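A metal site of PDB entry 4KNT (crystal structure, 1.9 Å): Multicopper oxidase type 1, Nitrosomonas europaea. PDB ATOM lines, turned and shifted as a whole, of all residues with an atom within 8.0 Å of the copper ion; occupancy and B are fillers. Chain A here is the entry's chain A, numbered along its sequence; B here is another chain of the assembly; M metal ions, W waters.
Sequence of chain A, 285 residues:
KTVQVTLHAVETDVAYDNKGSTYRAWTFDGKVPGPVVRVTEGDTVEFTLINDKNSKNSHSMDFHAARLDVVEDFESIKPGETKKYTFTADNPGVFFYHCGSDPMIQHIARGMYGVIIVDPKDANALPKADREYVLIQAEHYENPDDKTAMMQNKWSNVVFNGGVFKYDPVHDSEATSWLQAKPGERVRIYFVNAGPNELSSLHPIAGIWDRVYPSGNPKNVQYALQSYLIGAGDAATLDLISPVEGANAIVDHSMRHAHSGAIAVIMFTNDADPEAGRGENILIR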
ATOM      1  N   ASP A  62      -4.242 -15.964  24.400  1.00  0.00           N
ATOM      2  CA  ASP A  62      -5.440 -15.131  24.392  1.00  0.00           C
ATOM      3  C   ASP A  62      -6.591 -15.983  23.863  1.00  0.00           C
ATOM      4  O   ASP A  62      -6.554 -16.400  22.704  1.00  0.00           O
ATOM      5  CB  ASP A  62      -5.194 -13.909  23.499  1.00  0.00           C
ATOM      6  CG  ASP A  62      -6.417 -13.013  23.330  1.00  0.00           C
ATOM      7  OD1 ASP A  62      -7.571 -13.485  23.433  1.00  0.00           O
ATOM      8  OD2 ASP A  62      -6.205 -11.812  23.063  1.00  0.00           O
ATOM      9  N   PHE A  63      -7.594 -16.244  24.699  1.00  0.00           N
ATOM     10  CA  PHE A  63      -8.833 -16.908  24.282  1.00  0.00           C
ATOM     11  C   PHE A  63      -9.939 -15.870  24.112  1.00  0.00           C
ATOM     12  O   PHE A  63     -10.248 -15.137  25.056  1.00  0.00           O
ATOM     13  CB  PHE A  63      -9.309 -17.936  25.333  1.00  0.00           C
ATOM     14  CG  PHE A  63      -8.543 -19.241  25.339  1.00  0.00           C
ATOM     15  CD1 PHE A  63      -8.820 -20.229  24.393  1.00  0.00           C
ATOM     16  CD2 PHE A  63      -7.600 -19.503  26.328  1.00  0.00           C
ATOM     17  CE1 PHE A  63      -8.135 -21.449  24.413  1.00  0.00           C
ATOM     18  CE2 PHE A  63      -6.912 -20.717  26.363  1.00  0.00           C
ATOM     19  CZ  PHE A  63      -7.175 -21.698  25.398  1.00  0.00           C
ATOM     20  N   HIS A  64     -10.571 -15.824  22.939  1.00  0.00           N
ATOM     21  CA  HIS A  64     -11.730 -14.936  22.735  1.00  0.00           C
ATOM     22  C   HIS A  64     -12.966 -15.378  23.529  1.00  0.00           C
ATOM     23  O   HIS A  64     -13.962 -14.655  23.601  1.00  0.00           O
ATOM     24  CB  HIS A  64     -12.072 -14.823  21.245  1.00  0.00           C
ATOM     25  CG  HIS A  64     -11.161 -13.904  20.473  1.00  0.00           C
ATOM     26  ND1 HIS A  64     -11.523 -13.338  19.277  1.00  0.00           N
ATOM     27  CD2 HIS A  64      -9.916 -13.453  20.748  1.00  0.00           C
ATOM     28  CE1 HIS A  64     -10.537 -12.586  18.826  1.00  0.00           C
ATOM     29  NE2 HIS A  64      -9.544 -12.637  19.698  1.00  0.00           N
ATOM     30  N   PHE A  74      -3.133 -12.531  30.028  1.00  0.00           N
ATOM     31  CA  PHE A  74      -2.607 -12.720  28.674  1.00  0.00           C
ATOM     32  C   PHE A  74      -1.124 -12.317  28.539  1.00  0.00           C
ATOM     33  O   PHE A  74      -0.631 -12.129  27.424  1.00  0.00           O
ATOM     34  CB  PHE A  74      -3.460 -11.985  27.631  1.00  0.00           C
ATOM     35  CG  PHE A  74      -4.892 -12.476  27.525  1.00  0.00           C
ATOM     36  CD1 PHE A  74      -5.328 -13.607  28.223  1.00  0.00           C
ATOM     37  CD2 PHE A  74      -5.789 -11.830  26.686  1.00  0.00           C
ATOM     38  CE1 PHE A  74      -6.645 -14.062  28.117  1.00  0.00           C
ATOM     39  CE2 PHE A  74      -7.116 -12.277  26.566  1.00  0.00           C
ATOM     40  CZ  PHE A  74      -7.544 -13.392  27.281  1.00  0.00           C
ATOM     41  N   PHE A  96     -11.952 -17.499  18.415  1.00  0.00           N
ATOM     42  CA  PHE A  96     -10.549 -17.451  18.048  1.00  0.00           C
ATOM     43  C   PHE A  96      -9.695 -17.562  19.317  1.00  0.00           C
ATOM     44  O   PHE A  96     -10.028 -16.964  20.341  1.00  0.00           O
ATOM     45  CB  PHE A  96     -10.322 -16.094  17.364  1.00  0.00           C
ATOM     46  CG  PHE A  96      -8.951 -15.898  16.746  1.00  0.00           C
ATOM     47  CD1 PHE A  96      -8.153 -16.968  16.362  1.00  0.00           C
ATOM     48  CD2 PHE A  96      -8.487 -14.601  16.520  1.00  0.00           C
ATOM     49  CE1 PHE A  96      -6.902 -16.755  15.793  1.00  0.00           C
ATOM     50  CE2 PHE A  96      -7.233 -14.386  15.937  1.00  0.00           C
ATOM     51  CZ  PHE A  96      -6.444 -15.468  15.580  1.00  0.00           C
ATOM     52  N   TYR A  97      -8.631 -18.359  19.275  1.00  0.00           N
ATOM     53  CA  TYR A  97      -7.561 -18.229  20.253  1.00  0.00           C
ATOM     54  C   TYR A  97      -6.214 -18.062  19.563  1.00  0.00           C
ATOM     55  O   TYR A  97      -6.002 -18.580  18.467  1.00  0.00           O
ATOM     56  CB  TYR A  97      -7.557 -19.376  21.286  1.00  0.00           C
ATOM     57  CG  TYR A  97      -6.945 -20.710  20.885  1.00  0.00           C
ATOM     58  CD1 TYR A  97      -5.562 -20.846  20.700  1.00  0.00           C
ATOM     59  CD2 TYR A  97      -7.741 -21.850  20.751  1.00  0.00           C
ATOM     60  CE1 TYR A  97      -4.999 -22.067  20.364  1.00  0.00           C
ATOM     61  CE2 TYR A  97      -7.183 -23.080  20.413  1.00  0.00           C
ATOM     62  CZ  TYR A  97      -5.807 -23.186  20.224  1.00  0.00           C
ATOM     63  OH  TYR A  97      -5.240 -24.388  19.898  1.00  0.00           O
ATOM     64  N   HIS A  98      -5.321 -17.312  20.200  1.00  0.00           N
ATOM     65  CA  HIS A  98      -4.001 -17.020  19.622  1.00  0.00           C
ATOM     66  C   HIS A  98      -3.019 -16.524  20.665  1.00  0.00           C
ATOM     67  O   HIS A  98      -3.426 -16.124  21.760  1.00  0.00           O
ATOM     68  CB  HIS A  98      -4.128 -15.992  18.499  1.00  0.00           C
ATOM     69  CG  HIS A  98      -4.726 -14.685  18.927  1.00  0.00           C
ATOM     70  ND1 HIS A  98      -3.976 -13.647  19.437  1.00  0.00           N
ATOM     71  CD2 HIS A  98      -6.015 -14.254  18.926  1.00  0.00           C
ATOM     72  CE1 HIS A  98      -4.765 -12.636  19.735  1.00  0.00           C
ATOM     73  NE2 HIS A  98      -6.009 -12.972  19.425  1.00  0.00           N
ATOM     74  N   CYS A  99      -1.740 -16.573  20.332  1.00  0.00           N
ATOM     75  CA  CYS A  99      -0.705 -15.939  21.141  1.00  0.00           C
ATOM     76  C   CYS A  99      -0.908 -14.430  21.106  1.00  0.00           C
ATOM     77  O   CYS A  99      -1.235 -13.860  20.066  1.00  0.00           O
ATOM     78  CB  CYS A  99       0.684 -16.317  20.616  1.00  0.00           C
ATOM     79  SG  CYS A  99       2.050 -15.591  21.535  1.00  0.00           S
ATOM     80  N   GLY A 100      -0.737 -13.796  22.265  1.00  0.00           N
ATOM     81  CA  GLY A 100      -0.896 -12.348  22.379  1.00  0.00           C
ATOM     82  C   GLY A 100       0.417 -11.615  22.600  1.00  0.00           C
ATOM     83  O   GLY A 100       0.424 -10.475  23.088  1.00  0.00           O
ATOM     84  N   MET A 104       1.862  -9.161  17.999  1.00  0.00           N
ATOM     85  CA  MET A 104       0.814 -10.144  17.712  1.00  0.00           C
ATOM     86  C   MET A 104       0.714 -10.503  16.247  1.00  0.00           C
ATOM     87  O   MET A 104       0.470 -11.655  15.896  1.00  0.00           O
ATOM     88  CB  MET A 104      -0.543  -9.677  18.232  1.00  0.00           C
ATOM     89  CG  MET A 104      -0.744  -9.926  19.712  1.00  0.00           C
ATOM     90  SD  MET A 104      -2.435  -9.610  20.236  1.00  0.00           S
ATOM     91  CE  MET A 104      -2.414  -7.825  20.435  1.00  0.00           C
ATOM     92  N   ILE A 108       0.728 -14.525  15.395  1.00  0.00           N
ATOM     93  CA  ILE A 108      -0.397 -15.095  14.661  1.00  0.00           C
ATOM     94  C   ILE A 108       0.051 -15.628  13.288  1.00  0.00           C
ATOM     95  O   ILE A 108      -0.202 -16.780  12.957  1.00  0.00           O
ATOM     96  CB  ILE A 108      -1.574 -14.087  14.506  1.00  0.00           C
ATOM     97  CG1 ILE A 108      -2.188 -13.760  15.871  1.00  0.00           C
ATOM     98  CG2 ILE A 108      -2.657 -14.651  13.570  1.00  0.00           C
ATOM     99  CD1 ILE A 108      -3.193 -12.604  15.861  1.00  0.00           C
ATOM    100  N   ASN A 193     -11.426 -16.625  11.178  1.00  0.00           N
ATOM    101  CA  ASN A 193     -10.468 -15.842  10.395  1.00  0.00           C
ATOM    102  C   ASN A 193      -9.381 -15.314  11.320  1.00  0.00           C
ATOM    103  O   ASN A 193      -9.577 -14.336  12.031  1.00  0.00           O
ATOM    104  CB  ASN A 193     -11.157 -14.697   9.645  1.00  0.00           C
ATOM    105  CG  ASN A 193     -10.202 -13.932   8.730  1.00  0.00           C
ATOM    106  OD1 ASN A 193      -9.069 -14.354   8.486  1.00  0.00           O
ATOM    107  ND2 ASN A 193     -10.668 -12.811   8.210  1.00  0.00           N
ATOM    108  N   ALA A 194      -8.239 -15.999  11.310  1.00  0.00           N
ATOM    109  CA  ALA A 194      -7.104 -15.639  12.148  1.00  0.00           C
ATOM    110  C   ALA A 194      -6.386 -14.380  11.645  1.00  0.00           C
ATOM    111  O   ALA A 194      -5.702 -13.694  12.410  1.00  0.00           O
ATOM    112  CB  ALA A 194      -6.123 -16.811  12.246  1.00  0.00           C
ATOM    113  N   ALA A 232     -10.956  -9.963  10.361  1.00  0.00           N
ATOM    114  CA  ALA A 232      -9.780 -10.494  11.031  1.00  0.00           C
ATOM    115  C   ALA A 232     -10.082 -10.598  12.523  1.00  0.00           C
ATOM    116  O   ALA A 232     -10.586  -9.652  13.120  1.00  0.00           O
ATOM    117  CB  ALA A 232      -8.573  -9.602  10.782  1.00  0.00           C
ATOM    118  N   GLY A 233      -9.803 -11.768  13.096  1.00  0.00           N
ATOM    119  CA  GLY A 233     -10.047 -12.012  14.513  1.00  0.00           C
ATOM    120  C   GLY A 233     -11.491 -12.322  14.875  1.00  0.00           C
ATOM    121  O   GLY A 233     -11.874 -12.243  16.047  1.00  0.00           O
ATOM    122  N   ASP A 234     -12.299 -12.686  13.882  1.00  0.00           N
ATOM    123  CA  ASP A 234     -13.701 -13.032  14.124  1.00  0.00           C
ATOM    124  C   ASP A 234     -13.948 -14.492  13.755  1.00  0.00           C
ATOM    125  O   ASP A 234     -13.114 -15.129  13.108  1.00  0.00           O
ATOM    126  CB  ASP A 234     -14.639 -12.106  13.331  1.00  0.00           C
ATOM    127  CG  ASP A 234     -16.092 -12.170  13.803  1.00  0.00           C
ATOM    128  OD1 ASP A 234     -16.357 -12.550  14.969  1.00  0.00           O
ATOM    129  OD2 ASP A 234     -16.982 -11.849  12.996  1.00  0.00           O
ATOM    130  N   HIS B 203     -12.642  -5.485  18.442  1.00  0.00           N
ATOM    131  CA  HIS B 203     -12.618  -6.553  19.445  1.00  0.00           C
ATOM    132  C   HIS B 203     -12.059  -6.007  20.764  1.00  0.00           C
ATOM    133  O   HIS B 203     -11.068  -5.271  20.751  1.00  0.00           O
ATOM    134  CB  HIS B 203     -11.740  -7.707  18.940  1.00  0.00           C
ATOM    135  CG  HIS B 203     -11.392  -8.726  19.989  1.00  0.00           C
ATOM    136  ND1 HIS B 203     -12.287  -9.677  20.427  1.00  0.00           N
ATOM    137  CD2 HIS B 203     -10.248  -8.952  20.673  1.00  0.00           C
ATOM    138  CE1 HIS B 203     -11.712 -10.437  21.341  1.00  0.00           C
ATOM    139  NE2 HIS B 203     -10.475 -10.019  21.517  1.00  0.00           N
ATOM    140  N   PRO B 204     -12.704  -6.365  21.885  1.00  0.00           N
ATOM    141  CA  PRO B 204     -12.128  -6.042  23.184  1.00  0.00           C
ATOM    142  C   PRO B 204     -11.266  -7.205  23.684  1.00  0.00           C
ATOM    143  O   PRO B 204     -11.807  -8.251  24.082  1.00  0.00           O
ATOM    144  CB  PRO B 204     -13.372  -5.861  24.072  1.00  0.00           C
ATOM    145  CG  PRO B 204     -14.479  -6.621  23.381  1.00  0.00           C
ATOM    146  CD  PRO B 204     -13.995  -7.058  22.018  1.00  0.00           C
ATOM    147  N   ILE B 205      -9.945  -7.043  23.637  1.00  0.00           N
ATOM    148  CA  ILE B 205      -9.049  -8.090  24.121  1.00  0.00           C
ATOM    149  C   ILE B 205      -9.324  -8.363  25.594  1.00  0.00           C
ATOM    150  O   ILE B 205      -9.346  -7.434  26.404  1.00  0.00           O
ATOM    151  CB  ILE B 205      -7.546  -7.729  23.903  1.00  0.00           C
ATOM    152  CG1 ILE B 205      -7.268  -7.479  22.413  1.00  0.00           C
ATOM    153  CG2 ILE B 205      -6.652  -8.850  24.449  1.00  0.00           C
ATOM    154  CD1 ILE B 205      -5.808  -7.128  22.093  1.00  0.00           C
ATOM    155  N   ALA B 206      -9.551  -9.638  25.907  1.00  0.00           N
ATOM    156  CA  ALA B 206      -9.876 -10.129  27.259  1.00  0.00           C
ATOM    157  C   ALA B 206     -11.338  -9.915  27.644  1.00  0.00           C
ATOM    158  O   ALA B 206     -11.725 -10.119  28.800  1.00  0.00           O
ATOM    159  CB  ALA B 206      -8.923  -9.547  28.323  1.00  0.00           C
ATOM    160  N   GLN B 226     -17.531 -11.577  19.636  1.00  0.00           N
ATOM    161  CA  GLN B 226     -16.114 -11.367  19.912  1.00  0.00           C
ATOM    162  C   GLN B 226     -15.575 -10.193  19.106  1.00  0.00           C
ATOM    163  O   GLN B 226     -14.662  -9.496  19.545  1.00  0.00           O
ATOM    164  CB  GLN B 226     -15.302 -12.628  19.643  1.00  0.00           C
ATOM    165  CG  GLN B 226     -15.267 -13.075  18.192  1.00  0.00           C
ATOM    166  CD  GLN B 226     -14.969 -14.558  18.057  1.00  0.00           C
ATOM    167  OE1 GLN B 226     -13.831 -14.997  18.252  1.00  0.00           O
ATOM    168  NE2 GLN B 226     -15.994 -15.327  17.715  1.00  0.00           N
ATOM    169  N   SER B 227     -16.160  -9.996  17.930  1.00  0.00           N
ATOM    170  CA  SER B 227     -15.748  -8.936  17.025  1.00  0.00           C
ATOM    171  C   SER B 227     -16.935  -8.407  16.237  1.00  0.00           C
ATOM    172  O   SER B 227     -17.951  -9.093  16.095  1.00  0.00           O
ATOM    173  CB  SER B 227     -14.658  -9.439  16.073  1.00  0.00           C
ATOM    174  OG  SER B 227     -13.484  -9.786  16.782  1.00  0.00           O
ATOM    175  N   VAL B 251      -9.420  -3.037  20.308  1.00  0.00           N
ATOM    176  CA  VAL B 251      -8.529  -3.008  19.151  1.00  0.00           C
ATOM    177  C   VAL B 251      -9.279  -3.182  17.845  1.00  0.00           C
ATOM    178  O   VAL B 251     -10.363  -3.779  17.820  1.00  0.00           O
ATOM    179  CB  VAL B 251      -7.414  -4.105  19.235  1.00  0.00           C
ATOM    180  CG1 VAL B 251      -6.569  -3.931  20.489  1.00  0.00           C
ATOM    181  CG2 VAL B 251      -8.013  -5.519  19.173  1.00  0.00           C
ATOM    182  N   HIS B 253      -8.917  -5.463  15.095  1.00  0.00           N
ATOM    183  CA  HIS B 253      -8.231  -6.763  15.090  1.00  0.00           C
ATOM    184  C   HIS B 253      -7.481  -7.095  13.794  1.00  0.00           C
ATOM    185  O   HIS B 253      -6.812  -8.127  13.714  1.00  0.00           O
ATOM    186  CB  HIS B 253      -9.168  -7.900  15.505  1.00  0.00           C
ATOM    187  CG  HIS B 253      -8.474  -8.999  16.256  1.00  0.00           C
ATOM    188  ND1 HIS B 253      -7.479  -9.781  15.693  1.00  0.00           N
ATOM    189  CD2 HIS B 253      -8.640  -9.463  17.518  1.00  0.00           C
ATOM    190  CE1 HIS B 253      -7.065 -10.662  16.582  1.00  0.00           C
ATOM    191  NE2 HIS B 253      -7.748 -10.490  17.702  1.00  0.00           N
ATOM    192  N   MET B 255      -4.498  -6.723  12.503  1.00  0.00           N
ATOM    193  CA  MET B 255      -3.312  -6.403  13.321  1.00  0.00           C
ATOM    194  C   MET B 255      -2.461  -5.235  12.847  1.00  0.00           C
ATOM    195  O   MET B 255      -1.954  -4.477  13.682  1.00  0.00           O
ATOM    196  CB  MET B 255      -2.459  -7.653  13.592  1.00  0.00           C
ATOM    197  CG  MET B 255      -3.031  -8.579  14.679  1.00  0.00           C
ATOM    198  SD  MET B 255      -3.717  -7.790  16.173  1.00  0.00           S
ATOM    199  CE  MET B 255      -2.352  -6.845  16.811  1.00  0.00           C
HETATM  200 CU    CU M   1      -7.730 -11.865  19.291  1.00  0.00          CU
HETATM  201  O   HOH W   1      -7.613 -10.782  21.242  1.00  0.00           O
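NE2 of His 64 is bound to the copper ion (2.0 Å). A ring nitrogen (NE2) of His 98 is bound to the copper ion (2.1 Å). The copper ion is bound by a ring nitrogen (NE2) of His 253 of chain B, 2.1 Å away. Water W1 binds the copper ion (2.2 Å).
Residues that only touch the copper ion: Phe 96 and His 203 of chain B. Five residues have an atom within 4 Å of the copper ion: His 64, Phe 96, His 98, His 203 of chain B and His 253 of chain B. The nearest printed residue that does not touch the copper ion is Asp 62 (4.1 Å).
Water W1 bridges OD2 of Asp 62 and NE2 of His 203 of chain B.
A ring nitrogen (ND1) of His 64 lies close to the backbone carbonyl oxygen (O) of Gly 233, at 3.4 Å. O of Gln 226 of chain B sits at hydrogen-bond distance from ND1 of His 203 of chain B (2.5 Å). The backbone carbonyl oxygen (O) of His 98 is in hydrogen-bond range of the backbone NH (N) of Asp 62 (2.8 Å). N of His 64 lies within hydrogen-bond range of O of Phe 96 (2.9 Å). OE1 of Gln 226 of chain B sits at hydrogen-bond distance from N of Phe 96 (3.1 Å). ND1 of His 64 lies within hydrogen-bond range of OE1 of Gln 226 of chain B (3.0 Å). NE2 of His 64 lies close to NE2 of His 203 of chain B. The backbone carbonyl oxygen of His 203 of chain B lies within hydrogen-bond range of the backbone NH of Val 251 of chain B (2.8 Å).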
